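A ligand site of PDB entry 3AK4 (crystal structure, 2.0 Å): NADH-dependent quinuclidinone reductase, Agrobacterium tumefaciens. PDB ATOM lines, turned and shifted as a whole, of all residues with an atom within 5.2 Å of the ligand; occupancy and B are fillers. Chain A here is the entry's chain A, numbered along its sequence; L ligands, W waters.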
ATOM      1  N   GLY A  19     -31.329  -0.754  20.420  1.00  0.00           N
ATOM      2  CA  GLY A  19     -30.983  -2.180  20.315  1.00  0.00           C
ATOM      3  C   GLY A  19     -29.908  -2.594  21.306  1.00  0.00           C
ATOM      4  O   GLY A  19     -29.156  -3.546  21.052  1.00  0.00           O
ATOM      5  N   GLY A  20     -29.841  -1.886  22.433  1.00  0.00           N
ATOM      6  CA  GLY A  20     -28.803  -2.099  23.455  1.00  0.00           C
ATOM      7  C   GLY A  20     -29.106  -3.138  24.529  1.00  0.00           C
ATOM      8  O   GLY A  20     -28.327  -3.290  25.467  1.00  0.00           O
ATOM      9  N   SER A  21     -30.220  -3.854  24.397  1.00  0.00           N
ATOM     10  CA  SER A  21     -30.605  -4.858  25.417  1.00  0.00           C
ATOM     11  C   SER A  21     -29.753  -6.137  25.495  1.00  0.00           C
ATOM     12  O   SER A  21     -29.658  -6.750  26.549  1.00  0.00           O
ATOM     13  CB  SER A  21     -32.068  -5.278  25.239  1.00  0.00           C
ATOM     14  OG  SER A  21     -32.907  -4.274  25.793  1.00  0.00           O
ATOM     15  N   LYS A  22     -29.156  -6.541  24.376  1.00  0.00           N
ATOM     16  CA  LYS A  22     -28.429  -7.814  24.325  1.00  0.00           C
ATOM     17  C   LYS A  22     -27.352  -7.807  23.217  1.00  0.00           C
ATOM     18  O   LYS A  22     -27.297  -6.849  22.444  1.00  0.00           O
ATOM     19  CB  LYS A  22     -29.423  -8.991  24.157  1.00  0.00           C
ATOM     20  CG  LYS A  22     -30.287  -8.989  22.920  1.00  0.00           C
ATOM     21  CD  LYS A  22     -31.574  -9.850  23.078  1.00  0.00           C
ATOM     22  CE  LYS A  22     -32.642  -9.150  23.936  1.00  0.00           C
ATOM     23  NZ  LYS A  22     -33.932  -9.917  24.092  1.00  0.00           N
ATOM     24  N   GLY A  23     -26.517  -8.856  23.187  1.00  0.00           N
ATOM     25  CA  GLY A  23     -25.530  -9.060  22.103  1.00  0.00           C
ATOM     26  C   GLY A  23     -24.602  -7.871  21.874  1.00  0.00           C
ATOM     27  O   GLY A  23     -24.007  -7.322  22.822  1.00  0.00           O
ATOM     28  N   ILE A  24     -24.464  -7.461  20.609  1.00  0.00           N
ATOM     29  CA  ILE A  24     -23.598  -6.323  20.265  1.00  0.00           C
ATOM     30  C   ILE A  24     -23.976  -4.991  20.959  1.00  0.00           C
ATOM     31  O   ILE A  24     -23.104  -4.294  21.491  1.00  0.00           O
ATOM     32  CB  ILE A  24     -23.419  -6.129  18.715  1.00  0.00           C
ATOM     33  CG1 ILE A  24     -22.743  -7.382  18.130  1.00  0.00           C
ATOM     34  CG2 ILE A  24     -22.617  -4.824  18.420  1.00  0.00           C
ATOM     35  CD1 ILE A  24     -22.759  -7.440  16.592  1.00  0.00           C
ATOM     36  N   GLY A  25     -25.274  -4.672  20.961  1.00  0.00           N
ATOM     37  CA  GLY A  25     -25.792  -3.431  21.538  1.00  0.00           C
ATOM     38  C   GLY A  25     -25.486  -3.360  23.016  1.00  0.00           C
ATOM     39  O   GLY A  25     -25.110  -2.302  23.524  1.00  0.00           O
ATOM     40  N   ALA A  42     -32.524   2.266  24.395  1.00  0.00           N
ATOM     41  CA  ALA A  42     -33.872   2.140  23.836  1.00  0.00           C
ATOM     42  C   ALA A  42     -33.992   0.816  23.079  1.00  0.00           C
ATOM     43  O   ALA A  42     -33.255   0.584  22.132  1.00  0.00           O
ATOM     44  CB  ALA A  42     -34.174   3.316  22.928  1.00  0.00           C
ATOM     45  N   ASP A  43     -34.932  -0.032  23.497  1.00  0.00           N
ATOM     46  CA  ASP A  43     -35.025  -1.403  22.977  1.00  0.00           C
ATOM     47  C   ASP A  43     -36.463  -1.887  23.047  1.00  0.00           C
ATOM     48  O   ASP A  43     -37.260  -1.413  23.876  1.00  0.00           O
ATOM     49  CB  ASP A  43     -34.105  -2.361  23.763  1.00  0.00           C
ATOM     50  CG  ASP A  43     -33.752  -3.629  22.995  1.00  0.00           C
ATOM     51  OD1 ASP A  43     -34.564  -4.595  22.957  1.00  0.00           O
ATOM     52  OD2 ASP A  43     -32.621  -3.688  22.444  1.00  0.00           O
ATOM     53  N   LEU A  44     -36.780  -2.840  22.165  1.00  0.00           N
ATOM     54  CA  LEU A  44     -38.074  -3.562  22.162  1.00  0.00           C
ATOM     55  C   LEU A  44     -38.258  -4.371  23.460  1.00  0.00           C
ATOM     56  O   LEU A  44     -39.385  -4.545  23.940  1.00  0.00           O
ATOM     57  CB  LEU A  44     -38.139  -4.470  20.923  1.00  0.00           C
ATOM     58  CG  LEU A  44     -39.459  -4.979  20.341  1.00  0.00           C
ATOM     59  CD1 LEU A  44     -40.330  -3.814  19.825  1.00  0.00           C
ATOM     60  CD2 LEU A  44     -39.170  -5.973  19.202  1.00  0.00           C
ATOM     61  N   ASP A  45     -37.144  -4.857  24.014  1.00  0.00           N
ATOM     62  CA  ASP A  45     -37.146  -5.632  25.267  1.00  0.00           C
ATOM     63  C   ASP A  45     -36.629  -4.711  26.405  1.00  0.00           C
ATOM     64  O   ASP A  45     -35.412  -4.629  26.654  1.00  0.00           O
ATOM     65  CB  ASP A  45     -36.275  -6.879  25.095  1.00  0.00           C
ATOM     66  CG  ASP A  45     -36.291  -7.811  26.319  1.00  0.00           C
ATOM     67  OD1 ASP A  45     -36.703  -7.407  27.436  1.00  0.00           O
ATOM     68  OD2 ASP A  45     -35.841  -8.958  26.132  1.00  0.00           O
ATOM     69  N   VAL A  65     -38.747   1.069  22.985  1.00  0.00           N
ATOM     70  CA  VAL A  65     -38.880   1.646  21.634  1.00  0.00           C
ATOM     71  C   VAL A  65     -39.141   0.517  20.650  1.00  0.00           C
ATOM     72  O   VAL A  65     -38.707  -0.636  20.872  1.00  0.00           O
ATOM     73  CB  VAL A  65     -37.644   2.518  21.197  1.00  0.00           C
ATOM     74  CG1 VAL A  65     -36.495   1.586  20.726  1.00  0.00           C
ATOM     75  CG2 VAL A  65     -38.041   3.520  20.084  1.00  0.00           C
ATOM     76  N   ASP A  66     -39.892   0.836  19.604  1.00  0.00           N
ATOM     77  CA  ASP A  66     -39.970   0.046  18.381  1.00  0.00           C
ATOM     78  C   ASP A  66     -39.459   0.964  17.286  1.00  0.00           C
ATOM     79  O   ASP A  66     -40.163   1.899  16.868  1.00  0.00           O
ATOM     80  CB  ASP A  66     -41.418  -0.454  18.116  1.00  0.00           C
ATOM     81  CG  ASP A  66     -41.540  -1.332  16.875  1.00  0.00           C
ATOM     82  OD1 ASP A  66     -40.606  -1.355  16.039  1.00  0.00           O
ATOM     83  OD2 ASP A  66     -42.567  -2.041  16.735  1.00  0.00           O
ATOM     84  N   VAL A  67     -38.230   0.711  16.821  1.00  0.00           N
ATOM     85  CA  VAL A  67     -37.571   1.553  15.822  1.00  0.00           C
ATOM     86  C   VAL A  67     -38.246   1.530  14.446  1.00  0.00           C
ATOM     87  O   VAL A  67     -37.950   2.381  13.604  1.00  0.00           O
ATOM     88  CB  VAL A  67     -36.041   1.268  15.689  1.00  0.00           C
ATOM     89  CG1 VAL A  67     -35.306   1.464  17.051  1.00  0.00           C
ATOM     90  CG2 VAL A  67     -35.763  -0.133  15.094  1.00  0.00           C
ATOM     91  N   THR A  68     -39.154   0.567  14.203  1.00  0.00           N
ATOM     92  CA  THR A  68     -39.904   0.539  12.940  1.00  0.00           C
ATOM     93  C   THR A  68     -40.963   1.651  12.819  1.00  0.00           C
ATOM     94  O   THR A  68     -41.468   1.905  11.716  1.00  0.00           O
ATOM     95  CB  THR A  68     -40.597  -0.839  12.677  1.00  0.00           C
ATOM     96  OG1 THR A  68     -41.658  -1.054  13.620  1.00  0.00           O
ATOM     97  CG2 THR A  68     -39.601  -2.011  12.725  1.00  0.00           C
ATOM     98  N   ASN A  93     -28.156   0.606  16.637  1.00  0.00           N
ATOM     99  CA  ASN A  93     -27.687  -0.763  16.553  1.00  0.00           C
ATOM    100  C   ASN A  93     -28.790  -1.801  16.247  1.00  0.00           C
ATOM    101  O   ASN A  93     -28.478  -2.894  15.737  1.00  0.00           O
ATOM    102  CB  ASN A  93     -26.935  -1.103  17.870  1.00  0.00           C
ATOM    103  CG  ASN A  93     -26.636  -2.602  18.003  1.00  0.00           C
ATOM    104  OD1 ASN A  93     -27.338  -3.345  18.694  1.00  0.00           O
ATOM    105  ND2 ASN A  93     -25.599  -3.042  17.313  1.00  0.00           N
ATOM    106  N   ALA A  94     -30.052  -1.483  16.543  1.00  0.00           N
ATOM    107  CA  ALA A  94     -31.131  -2.484  16.454  1.00  0.00           C
ATOM    108  C   ALA A  94     -31.143  -3.080  15.040  1.00  0.00           C
ATOM    109  O   ALA A  94     -31.016  -2.359  14.030  1.00  0.00           O
ATOM    110  CB  ALA A  94     -32.507  -1.860  16.783  1.00  0.00           C
ATOM    111  N   GLY A  95     -31.223  -4.400  14.970  1.00  0.00           N
ATOM    112  CA  GLY A  95     -31.292  -5.114  13.699  1.00  0.00           C
ATOM    113  C   GLY A  95     -31.829  -6.520  13.861  1.00  0.00           C
ATOM    114  O   GLY A  95     -31.801  -7.090  14.973  1.00  0.00           O
ATOM    115  N   VAL A  96     -32.344  -7.071  12.751  1.00  0.00           N
ATOM    116  CA  VAL A  96     -32.853  -8.436  12.678  1.00  0.00           C
ATOM    117  C   VAL A  96     -32.404  -9.158  11.397  1.00  0.00           C
ATOM    118  O   VAL A  96     -31.910  -8.513  10.450  1.00  0.00           O
ATOM    119  CB  VAL A  96     -34.393  -8.443  12.718  1.00  0.00           C
ATOM    120  CG1 VAL A  96     -34.906  -7.851  14.064  1.00  0.00           C
ATOM    121  CG2 VAL A  96     -34.967  -7.661  11.501  1.00  0.00           C
ATOM    122  N   VAL A 116     -36.886  -2.795  10.261  1.00  0.00           N
ATOM    123  CA  VAL A 116     -35.933  -2.713  11.383  1.00  0.00           C
ATOM    124  C   VAL A 116     -34.558  -2.152  10.965  1.00  0.00           C
ATOM    125  O   VAL A 116     -34.098  -1.132  11.503  1.00  0.00           O
ATOM    126  CB  VAL A 116     -35.793  -4.020  12.219  1.00  0.00           C
ATOM    127  CG1 VAL A 116     -34.826  -3.810  13.399  1.00  0.00           C
ATOM    128  CG2 VAL A 116     -37.187  -4.516  12.758  1.00  0.00           C
ATOM    129  N   ASN A 117     -33.898  -2.811  10.019  1.00  0.00           N
ATOM    130  CA  ASN A 117     -32.502  -2.496   9.704  1.00  0.00           C
ATOM    131  C   ASN A 117     -32.288  -1.156   9.027  1.00  0.00           C
ATOM    132  O   ASN A 117     -31.381  -0.419   9.421  1.00  0.00           O
ATOM    133  CB  ASN A 117     -31.825  -3.612   8.844  1.00  0.00           C
ATOM    134  CG  ASN A 117     -31.911  -4.971   9.494  1.00  0.00           C
ATOM    135  OD1 ASN A 117     -32.175  -5.088  10.694  1.00  0.00           O
ATOM    136  ND2 ASN A 117     -31.734  -6.036   8.698  1.00  0.00           N
ATOM    137  N   THR A 144     -24.776   0.478  13.236  1.00  0.00           N
ATOM    138  CA  THR A 144     -24.344  -0.911  13.056  1.00  0.00           C
ATOM    139  C   THR A 144     -24.887  -1.482  11.736  1.00  0.00           C
ATOM    140  O   THR A 144     -26.092  -1.745  11.595  1.00  0.00           O
ATOM    141  CB  THR A 144     -24.752  -1.833  14.240  1.00  0.00           C
ATOM    142  OG1 THR A 144     -24.340  -1.258  15.485  1.00  0.00           O
ATOM    143  CG2 THR A 144     -24.117  -3.265  14.086  1.00  0.00           C
ATOM    144  N   ALA A 145     -24.004  -1.590  10.749  1.00  0.00           N
ATOM    145  CA  ALA A 145     -24.361  -2.183   9.487  1.00  0.00           C
ATOM    146  C   ALA A 145     -23.985  -3.670   9.538  1.00  0.00           C
ATOM    147  O   ALA A 145     -24.432  -4.411  10.453  1.00  0.00           O
ATOM    148  CB  ALA A 145     -23.646  -1.399   8.306  1.00  0.00           C
ATOM    149  N   SER A 146     -23.142  -4.119   8.623  1.00  0.00           N
ATOM    150  CA  SER A 146     -22.746  -5.535   8.563  1.00  0.00           C
ATOM    151  C   SER A 146     -21.681  -5.758   7.502  1.00  0.00           C
ATOM    152  O   SER A 146     -21.546  -4.951   6.576  1.00  0.00           O
ATOM    153  CB  SER A 146     -23.997  -6.377   8.183  1.00  0.00           C
ATOM    154  OG  SER A 146     -23.740  -7.739   8.011  1.00  0.00           O
ATOM    155  N   LEU A 147     -20.937  -6.867   7.625  1.00  0.00           N
ATOM    156  CA  LEU A 147     -20.207  -7.446   6.477  1.00  0.00           C
ATOM    157  C   LEU A 147     -21.090  -7.516   5.215  1.00  0.00           C
ATOM    158  O   LEU A 147     -20.623  -7.217   4.102  1.00  0.00           O
ATOM    159  CB  LEU A 147     -19.662  -8.842   6.806  1.00  0.00           C
ATOM    160  CG  LEU A 147     -18.993  -9.690   5.688  1.00  0.00           C
ATOM    161  CD1 LEU A 147     -17.789  -8.972   5.129  1.00  0.00           C
ATOM    162  CD2 LEU A 147     -18.597 -11.076   6.196  1.00  0.00           C
ATOM    163  N   TYR A 159     -31.643  -9.393   3.580  1.00  0.00           N
ATOM    164  CA  TYR A 159     -30.815  -8.833   4.669  1.00  0.00           C
ATOM    165  C   TYR A 159     -29.653  -7.977   4.115  1.00  0.00           C
ATOM    166  O   TYR A 159     -29.447  -6.871   4.592  1.00  0.00           O
ATOM    167  CB  TYR A 159     -30.246  -9.955   5.542  1.00  0.00           C
ATOM    168  CG  TYR A 159     -29.342  -9.509   6.671  1.00  0.00           C
ATOM    169  CD1 TYR A 159     -29.884  -9.062   7.890  1.00  0.00           C
ATOM    170  CD2 TYR A 159     -27.933  -9.597   6.549  1.00  0.00           C
ATOM    171  CE1 TYR A 159     -29.065  -8.667   8.939  1.00  0.00           C
ATOM    172  CE2 TYR A 159     -27.095  -9.207   7.593  1.00  0.00           C
ATOM    173  CZ  TYR A 159     -27.660  -8.730   8.780  1.00  0.00           C
ATOM    174  OH  TYR A 159     -26.855  -8.373   9.820  1.00  0.00           O
ATOM    175  N   LYS A 163     -28.881  -3.848   4.570  1.00  0.00           N
ATOM    176  CA  LYS A 163     -27.657  -3.402   5.222  1.00  0.00           C
ATOM    177  C   LYS A 163     -26.826  -2.513   4.275  1.00  0.00           C
ATOM    178  O   LYS A 163     -26.207  -1.544   4.740  1.00  0.00           O
ATOM    179  CB  LYS A 163     -26.833  -4.603   5.729  1.00  0.00           C
ATOM    180  CG  LYS A 163     -27.438  -5.331   6.963  1.00  0.00           C
ATOM    181  CD  LYS A 163     -27.519  -4.360   8.162  1.00  0.00           C
ATOM    182  CE  LYS A 163     -27.729  -5.143   9.459  1.00  0.00           C
ATOM    183  NZ  LYS A 163     -27.874  -4.220  10.605  1.00  0.00           N
ATOM    184  N   PRO A 189     -19.623  -5.478  11.211  1.00  0.00           N
ATOM    185  CA  PRO A 189     -19.092  -6.656  11.910  1.00  0.00           C
ATOM    186  C   PRO A 189     -19.051  -7.947  11.045  1.00  0.00           C
ATOM    187  O   PRO A 189     -19.768  -8.050  10.069  1.00  0.00           O
ATOM    188  CB  PRO A 189     -20.053  -6.833  13.107  1.00  0.00           C
ATOM    189  CG  PRO A 189     -20.773  -5.549  13.236  1.00  0.00           C
ATOM    190  CD  PRO A 189     -20.874  -5.007  11.814  1.00  0.00           C
ATOM    191  N   GLY A 190     -18.221  -8.918  11.447  1.00  0.00           N
ATOM    192  CA  GLY A 190     -18.154 -10.215  10.771  1.00  0.00           C
ATOM    193  C   GLY A 190     -19.055 -11.264  11.406  1.00  0.00           C
ATOM    194  O   GLY A 190     -20.254 -11.054  11.557  1.00  0.00           O
ATOM    195  N   PHE A 191     -18.465 -12.407  11.771  1.00  0.00           N
ATOM    196  CA  PHE A 191     -19.264 -13.518  12.305  1.00  0.00           C
ATOM    197  C   PHE A 191     -19.262 -13.469  13.843  1.00  0.00           C
ATOM    198  O   PHE A 191     -18.487 -14.177  14.510  1.00  0.00           O
ATOM    199  CB  PHE A 191     -18.738 -14.879  11.766  1.00  0.00           C
ATOM    200  CG  PHE A 191     -18.557 -14.923  10.250  1.00  0.00           C
ATOM    201  CD1 PHE A 191     -19.652 -14.819   9.365  1.00  0.00           C
ATOM    202  CD2 PHE A 191     -17.279 -15.107   9.697  1.00  0.00           C
ATOM    203  CE1 PHE A 191     -19.458 -14.852   7.948  1.00  0.00           C
ATOM    204  CE2 PHE A 191     -17.079 -15.139   8.301  1.00  0.00           C
ATOM    205  CZ  PHE A 191     -18.183 -15.040   7.425  1.00  0.00           C
ATOM    206  N   VAL A 192     -20.157 -12.654  14.404  1.00  0.00           N
ATOM    207  CA  VAL A 192     -20.184 -12.397  15.853  1.00  0.00           C
ATOM    208  C   VAL A 192     -21.054 -13.391  16.641  1.00  0.00           C
ATOM    209  O   VAL A 192     -22.263 -13.562  16.363  1.00  0.00           O
ATOM    210  CB  VAL A 192     -20.610 -10.949  16.170  1.00  0.00           C
ATOM    211  CG1 VAL A 192     -20.486 -10.636  17.663  1.00  0.00           C
ATOM    212  CG2 VAL A 192     -19.802  -9.979  15.350  1.00  0.00           C
ATOM    213  N   THR A 194     -23.339 -14.307  19.014  1.00  0.00           N
ATOM    214  CA  THR A 194     -24.488 -13.789  19.789  1.00  0.00           C
ATOM    215  C   THR A 194     -25.668 -14.759  19.521  1.00  0.00           C
ATOM    216  O   THR A 194     -25.471 -15.792  18.896  1.00  0.00           O
ATOM    217  CB  THR A 194     -24.969 -12.414  19.267  1.00  0.00           C
ATOM    218  OG1 THR A 194     -25.575 -12.582  17.976  1.00  0.00           O
ATOM    219  CG2 THR A 194     -23.808 -11.350  19.206  1.00  0.00           C
ATOM    220  N   ALA A 195     -26.888 -14.401  19.948  1.00  0.00           N
ATOM    221  CA  ALA A 195     -28.091 -15.172  19.654  1.00  0.00           C
ATOM    222  C   ALA A 195     -28.410 -15.214  18.141  1.00  0.00           C
ATOM    223  O   ALA A 195     -28.969 -16.187  17.661  1.00  0.00           O
ATOM    224  CB  ALA A 195     -29.241 -14.663  20.435  1.00  0.00           C
ATOM    225  N   MET A 196     -28.048 -14.158  17.415  1.00  0.00           N
ATOM    226  CA  MET A 196     -28.263 -14.139  15.966  1.00  0.00           C
ATOM    227  C   MET A 196     -27.441 -15.238  15.275  1.00  0.00           C
ATOM    228  O   MET A 196     -27.976 -16.007  14.459  1.00  0.00           O
ATOM    229  CB  MET A 196     -27.963 -12.759  15.350  1.00  0.00           C
ATOM    230  CG  MET A 196     -28.290 -12.683  13.838  1.00  0.00           C
ATOM    231  SD  MET A 196     -28.227 -11.025  13.131  1.00  0.00           S
ATOM    232  CE  MET A 196     -29.537 -10.207  14.077  1.00  0.00           C
ATOM    233  N   GLN A 197     -26.157 -15.310  15.615  1.00  0.00           N
ATOM    234  CA  GLN A 197     -25.324 -16.395  15.122  1.00  0.00           C
ATOM    235  C   GLN A 197     -25.918 -17.792  15.442  1.00  0.00           C
ATOM    236  O   GLN A 197     -26.016 -18.632  14.555  1.00  0.00           O
ATOM    237  CB  GLN A 197     -23.878 -16.296  15.636  1.00  0.00           C
ATOM    238  CG  GLN A 197     -22.984 -17.388  15.067  1.00  0.00           C
ATOM    239  CD  GLN A 197     -21.522 -17.192  15.396  1.00  0.00           C
ATOM    240  OE1 GLN A 197     -20.861 -16.313  14.822  1.00  0.00           O
ATOM    241  NE2 GLN A 197     -20.997 -18.037  16.309  1.00  0.00           N
ATOM    242  N   ARG A 199     -29.020 -18.870  16.051  1.00  0.00           N
ATOM    243  CA  ARG A 199     -30.187 -19.089  15.183  1.00  0.00           C
ATOM    244  C   ARG A 199     -29.728 -19.391  13.763  1.00  0.00           C
ATOM    245  O   ARG A 199     -30.155 -20.388  13.134  1.00  0.00           O
ATOM    246  CB  ARG A 199     -31.083 -17.829  15.124  1.00  0.00           C
ATOM    247  CG  ARG A 199     -31.789 -17.402  16.433  1.00  0.00           C
ATOM    248  CD  ARG A 199     -32.902 -16.344  16.156  1.00  0.00           C
ATOM    249  NE  ARG A 199     -32.351 -14.995  15.921  1.00  0.00           N
ATOM    250  CZ  ARG A 199     -32.025 -14.125  16.881  1.00  0.00           C
ATOM    251  NH1 ARG A 199     -32.199 -14.425  18.164  1.00  0.00           N
ATOM    252  NH2 ARG A 199     -31.527 -12.931  16.559  1.00  0.00           N
ATOM    253  N   GLU A 200     -28.846 -18.532  13.256  1.00  0.00           N
ATOM    254  CA  GLU A 200     -28.439 -18.574  11.865  1.00  0.00           C
ATOM    255  C   GLU A 200     -27.671 -19.835  11.514  1.00  0.00           C
ATOM    256  O   GLU A 200     -27.806 -20.351  10.400  1.00  0.00           O
ATOM    257  CB  GLU A 200     -27.616 -17.338  11.461  1.00  0.00           C
ATOM    258  CG  GLU A 200     -28.473 -16.103  11.061  1.00  0.00           C
ATOM    259  CD  GLU A 200     -27.643 -14.856  10.772  1.00  0.00           C
ATOM    260  OE1 GLU A 200     -26.394 -14.928  10.856  1.00  0.00           O
ATOM    261  OE2 GLU A 200     -28.248 -13.791  10.471  1.00  0.00           O
HETATM  262  P1  LIG L   1     -29.576  -9.763  18.708  1.00  0.00           P
HETATM  263  O1  LIG L   1     -30.724 -10.461  18.024  1.00  0.00           O
HETATM  264  O2  LIG L   1     -28.863 -10.414  19.858  1.00  0.00           O
HETATM  265  O3  LIG L   1     -30.024  -8.313  19.234  1.00  0.00           O
HETATM  266  C1  LIG L   1     -30.772  -7.337  18.492  1.00  0.00           C
HETATM  267  C2  LIG L   1     -31.224  -6.227  19.482  1.00  0.00           C
HETATM  268  O4  LIG L   1     -32.063  -5.284  18.765  1.00  0.00           O
HETATM  269  C3  LIG L   1     -32.071  -6.809  20.638  1.00  0.00           C
HETATM  270  O5  LIG L   1     -31.798  -6.150  21.916  1.00  0.00           O
HETATM  271  C4  LIG L   1     -33.506  -6.557  20.160  1.00  0.00           C
HETATM  272  O6  LIG L   1     -34.467  -6.419  21.218  1.00  0.00           O
HETATM  273  C5  LIG L   1     -33.353  -5.251  19.357  1.00  0.00           C
HETATM  274  N1  LIG L   1     -34.477  -5.018  18.390  1.00  0.00           N
HETATM  275  C6  LIG L   1     -34.939  -5.828  17.425  1.00  0.00           C
HETATM  276  N2  LIG L   1     -35.974  -5.214  16.825  1.00  0.00           N
HETATM  277  C7  LIG L   1     -36.144  -4.021  17.447  1.00  0.00           C
HETATM  278  C8  LIG L   1     -37.046  -2.990  17.245  1.00  0.00           C
HETATM  279  N3  LIG L   1     -37.998  -3.132  16.255  1.00  0.00           N
HETATM  280  N4  LIG L   1     -36.938  -1.895  18.049  1.00  0.00           N
HETATM  281  C9  LIG L   1     -35.993  -1.773  19.003  1.00  0.00           C
HETATM  282  N5  LIG L   1     -35.133  -2.786  19.227  1.00  0.00           N
HETATM  283  C10 LIG L   1     -35.202  -3.905  18.431  1.00  0.00           C
HETATM  284  O7  LIG L   1     -28.502  -9.446  17.528  1.00  0.00           O
HETATM  285  P2  LIG L   1     -26.909  -9.099  17.496  1.00  0.00           P
HETATM  286  O8  LIG L   1     -26.351  -8.421  18.725  1.00  0.00           O
HETATM  287  O9  LIG L   1     -26.273 -10.315  16.886  1.00  0.00           O
HETATM  288  O10 LIG L   1     -27.001  -7.976  16.331  1.00  0.00           O
HETATM  289  C11 LIG L   1     -26.909  -6.555  16.587  1.00  0.00           C
HETATM  290  C12 LIG L   1     -26.684  -5.774  15.272  1.00  0.00           C
HETATM  291  O11 LIG L   1     -25.509  -6.257  14.614  1.00  0.00           O
HETATM  292  C13 LIG L   1     -27.843  -5.936  14.269  1.00  0.00           C
HETATM  293  O12 LIG L   1     -28.013  -4.665  13.617  1.00  0.00           O
HETATM  294  C14 LIG L   1     -27.328  -7.034  13.328  1.00  0.00           C
HETATM  295  O13 LIG L   1     -27.919  -6.986  12.008  1.00  0.00           O
HETATM  296  C15 LIG L   1     -25.823  -6.732  13.302  1.00  0.00           C
HETATM  297  N6  LIG L   1     -24.908  -7.812  12.929  1.00  0.00           N
HETATM  298  C16 LIG L   1     -24.782  -8.962  13.634  1.00  0.00           C
HETATM  299  C17 LIG L   1     -23.846  -9.953  13.237  1.00  0.00           C
HETATM  300  C18 LIG L   1     -23.691 -11.301  13.952  1.00  0.00           C
HETATM  301  O14 LIG L   1     -23.005 -12.183  13.417  1.00  0.00           O
HETATM  302  N7  LIG L   1     -24.335 -11.572  15.097  1.00  0.00           N
HETATM  303  C19 LIG L   1     -23.066  -9.673  12.096  1.00  0.00           C
HETATM  304  C20 LIG L   1     -23.216  -8.480  11.378  1.00  0.00           C
HETATM  305  C21 LIG L   1     -24.152  -7.548  11.832  1.00  0.00           C
HETATM  306  O   HOH W   1     -22.265 -14.895  12.869  1.00  0.00           O
HETATM  307  O   HOH W   2     -39.844  -5.292  14.673  1.00  0.00           O
HETATM  308  O   HOH W   3     -27.509  -6.420  19.685  1.00  0.00           O
HETATM  309  O   HOH W   4     -32.351  -9.641  16.053  1.00  0.00           O
HETATM  310  O   HOH W   5     -31.885 -12.155  19.940  1.00  0.00           O
HETATM  311  O   HOH W   6     -37.932  -6.833  15.679  1.00  0.00           O
HETATM  312  O   HOH W   7     -27.776 -11.936  21.562  1.00  0.00           O
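CA of Gly 19 touches O4 of the ligand, 3.6 Å away.
CB of Ser 21 touches O5 of the ligand, at 3.4 Å.
Lys 22 touches the ligand (CG to O5, 3.4 Å).
Gly 23 touches the ligand.
Val 65 touches the ligand.
Ala 94 touches the ligand.
Val 96 touches the ligand (CG1 to C6, 3.9 Å).
Val 116 touches the ligand (CG2 to N3, 3.8 Å).
CG2 of Thr 144 touches O11 of the ligand, 3.3 Å away.
Ala 145 touches the ligand (O to C21, 3.4 Å).
OG of Ser 146 touches C20 of the ligand, at 3.5 Å.
Pro 189 touches the ligand (O to C20, 3.7 Å).
Gly 190 touches the ligand.
C of Phe 191 touches O14 of the ligand, 3.98 Å away.
Met 196 touches the ligand (CB to O9, 3.3 Å).
Hydrophobic or aromatic side chains within 4 Å of the ligand: Ile 24, Leu 44, Val 65, Val 67, Ala 94, Val 96, Val 116, Tyr 159, Pro 189, Val 192 and Met 196.
27 residues have an atom within 4 Å of the ligand: Gly 19, Ser 21, Lys 22, Gly 23, Ile 24, Asp 43, Leu 44, Val 65, Asp 66, Val 67, Asn 93, Ala 94, Gly 95, Val 96, Val 116, Thr 144, Ala 145, Ser 146, Tyr 159, Lys 163, Pro 189, Gly 190, Phe 191, Val 192, Thr 194, Met 196 and Arg 199.
The side-chain carboxylate (OD1) of Asp 43 is in hydrogen-bond range of the backbone NH (N) of Asp 45, 2.8 Å away.
The side-chain carboxylate (OD2) of Asp 43 sits at hydrogen-bond distance from the backbone NH (N) of Ser 21, at 3.1 Å.
OD1 of Asn 93 sits close to N of Gly 25 (3.3 Å).
O of Ala 145 sits at hydrogen-bond distance from NZ of Lys 163, at 3.5 Å.
The backbone NH of Val 96 sits at hydrogen-bond distance from the side-chain amide oxygen of Asn 117.
The backbone carbonyl oxygen of Phe 191 lies close to the side-chain amide oxygen of Gln 197, at 3.2 Å.
OD1 of Asn 93 sits close to O of Gly 19 (3.0 Å).
N of Met 196 is in hydrogen-bond range of OG1 of Thr 194, 3.0 Å away.
The side-chain carboxylate (OD1) of Asp 43 is in hydrogen-bond range of an oxygen (O6) of the ligand, at 2.5 Å.
N4 of the ligand sits at hydrogen-bond distance from N of Val 67 (3.2 Å).
N of Val 192 sits at hydrogen-bond distance from O14 of the ligand.
The backbone NH of Gly 95 sits close to an oxygen (O12) of the ligand.
N of Ile 24 is in hydrogen-bond range of O8 of the ligand, at 2.8 Å.
An oxygen (O12) of the ligand lies within hydrogen-bond range of the backbone carbonyl oxygen (O) of Asn 93, 2.8 Å away.
The side-chain amino group (NZ) of Lys 163 is in hydrogen-bond range of an oxygen (O12) of the ligand, at 3.0 Å.
An oxygen (O9) of the ligand is in hydrogen-bond range of the side-chain hydroxyl of Thr 194 (2.6 Å).
The side-chain hydroxyl (OH) of Tyr 159 lies within hydrogen-bond range of an oxygen (O13) of the ligand, 2.8 Å away.
A nitrogen (N7) of the ligand is in hydrogen-bond range of the backbone carbonyl oxygen (O) of Val 192 (3.1 Å).
NH2 of Arg 199 lies within salt-bridge range of O1 of the ligand, at 3.0 Å.
The backbone NH (N) of Leu 44 sits at hydrogen-bond distance from a nitrogen (N5) of the ligand, at 3.4 Å.
A nitrogen (N3) of the ligand lies within hydrogen-bond range of the side-chain carboxylate (OD1) of Asp 66 (3.2 Å).
Water W3 lies within hydrogen-bond range of an oxygen (O8) of the ligand, the backbone carbonyl oxygen (O) of Lys 22, the backbone NH (N) of Gly 25, the side-chain amide oxygen (OD1) of Asn 93 and the backbone NH (N) of Ile 24.
Water W7 bridges an oxygen (O2) of the ligand and the backbone NH of Ala 195.
Water W4 lies within hydrogen-bond range of O1 of the ligand (2.7 Å), O of Gly 95 (2.8 Å) and NH2 of Arg 199 (3.4 Å).
Water W5 lies within hydrogen-bond range of an oxygen (O1) of the ligand (2.8 Å) and the guanidinium group of Arg 199 (2.9 Å).
Water W1 lies within hydrogen-bond range of the side-chain amide oxygen (OE1) of Gln 197 (2.8 Å), an oxygen (O14) of the ligand (2.9 Å) and the backbone NH (N) of Val 192 (3.4 Å).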
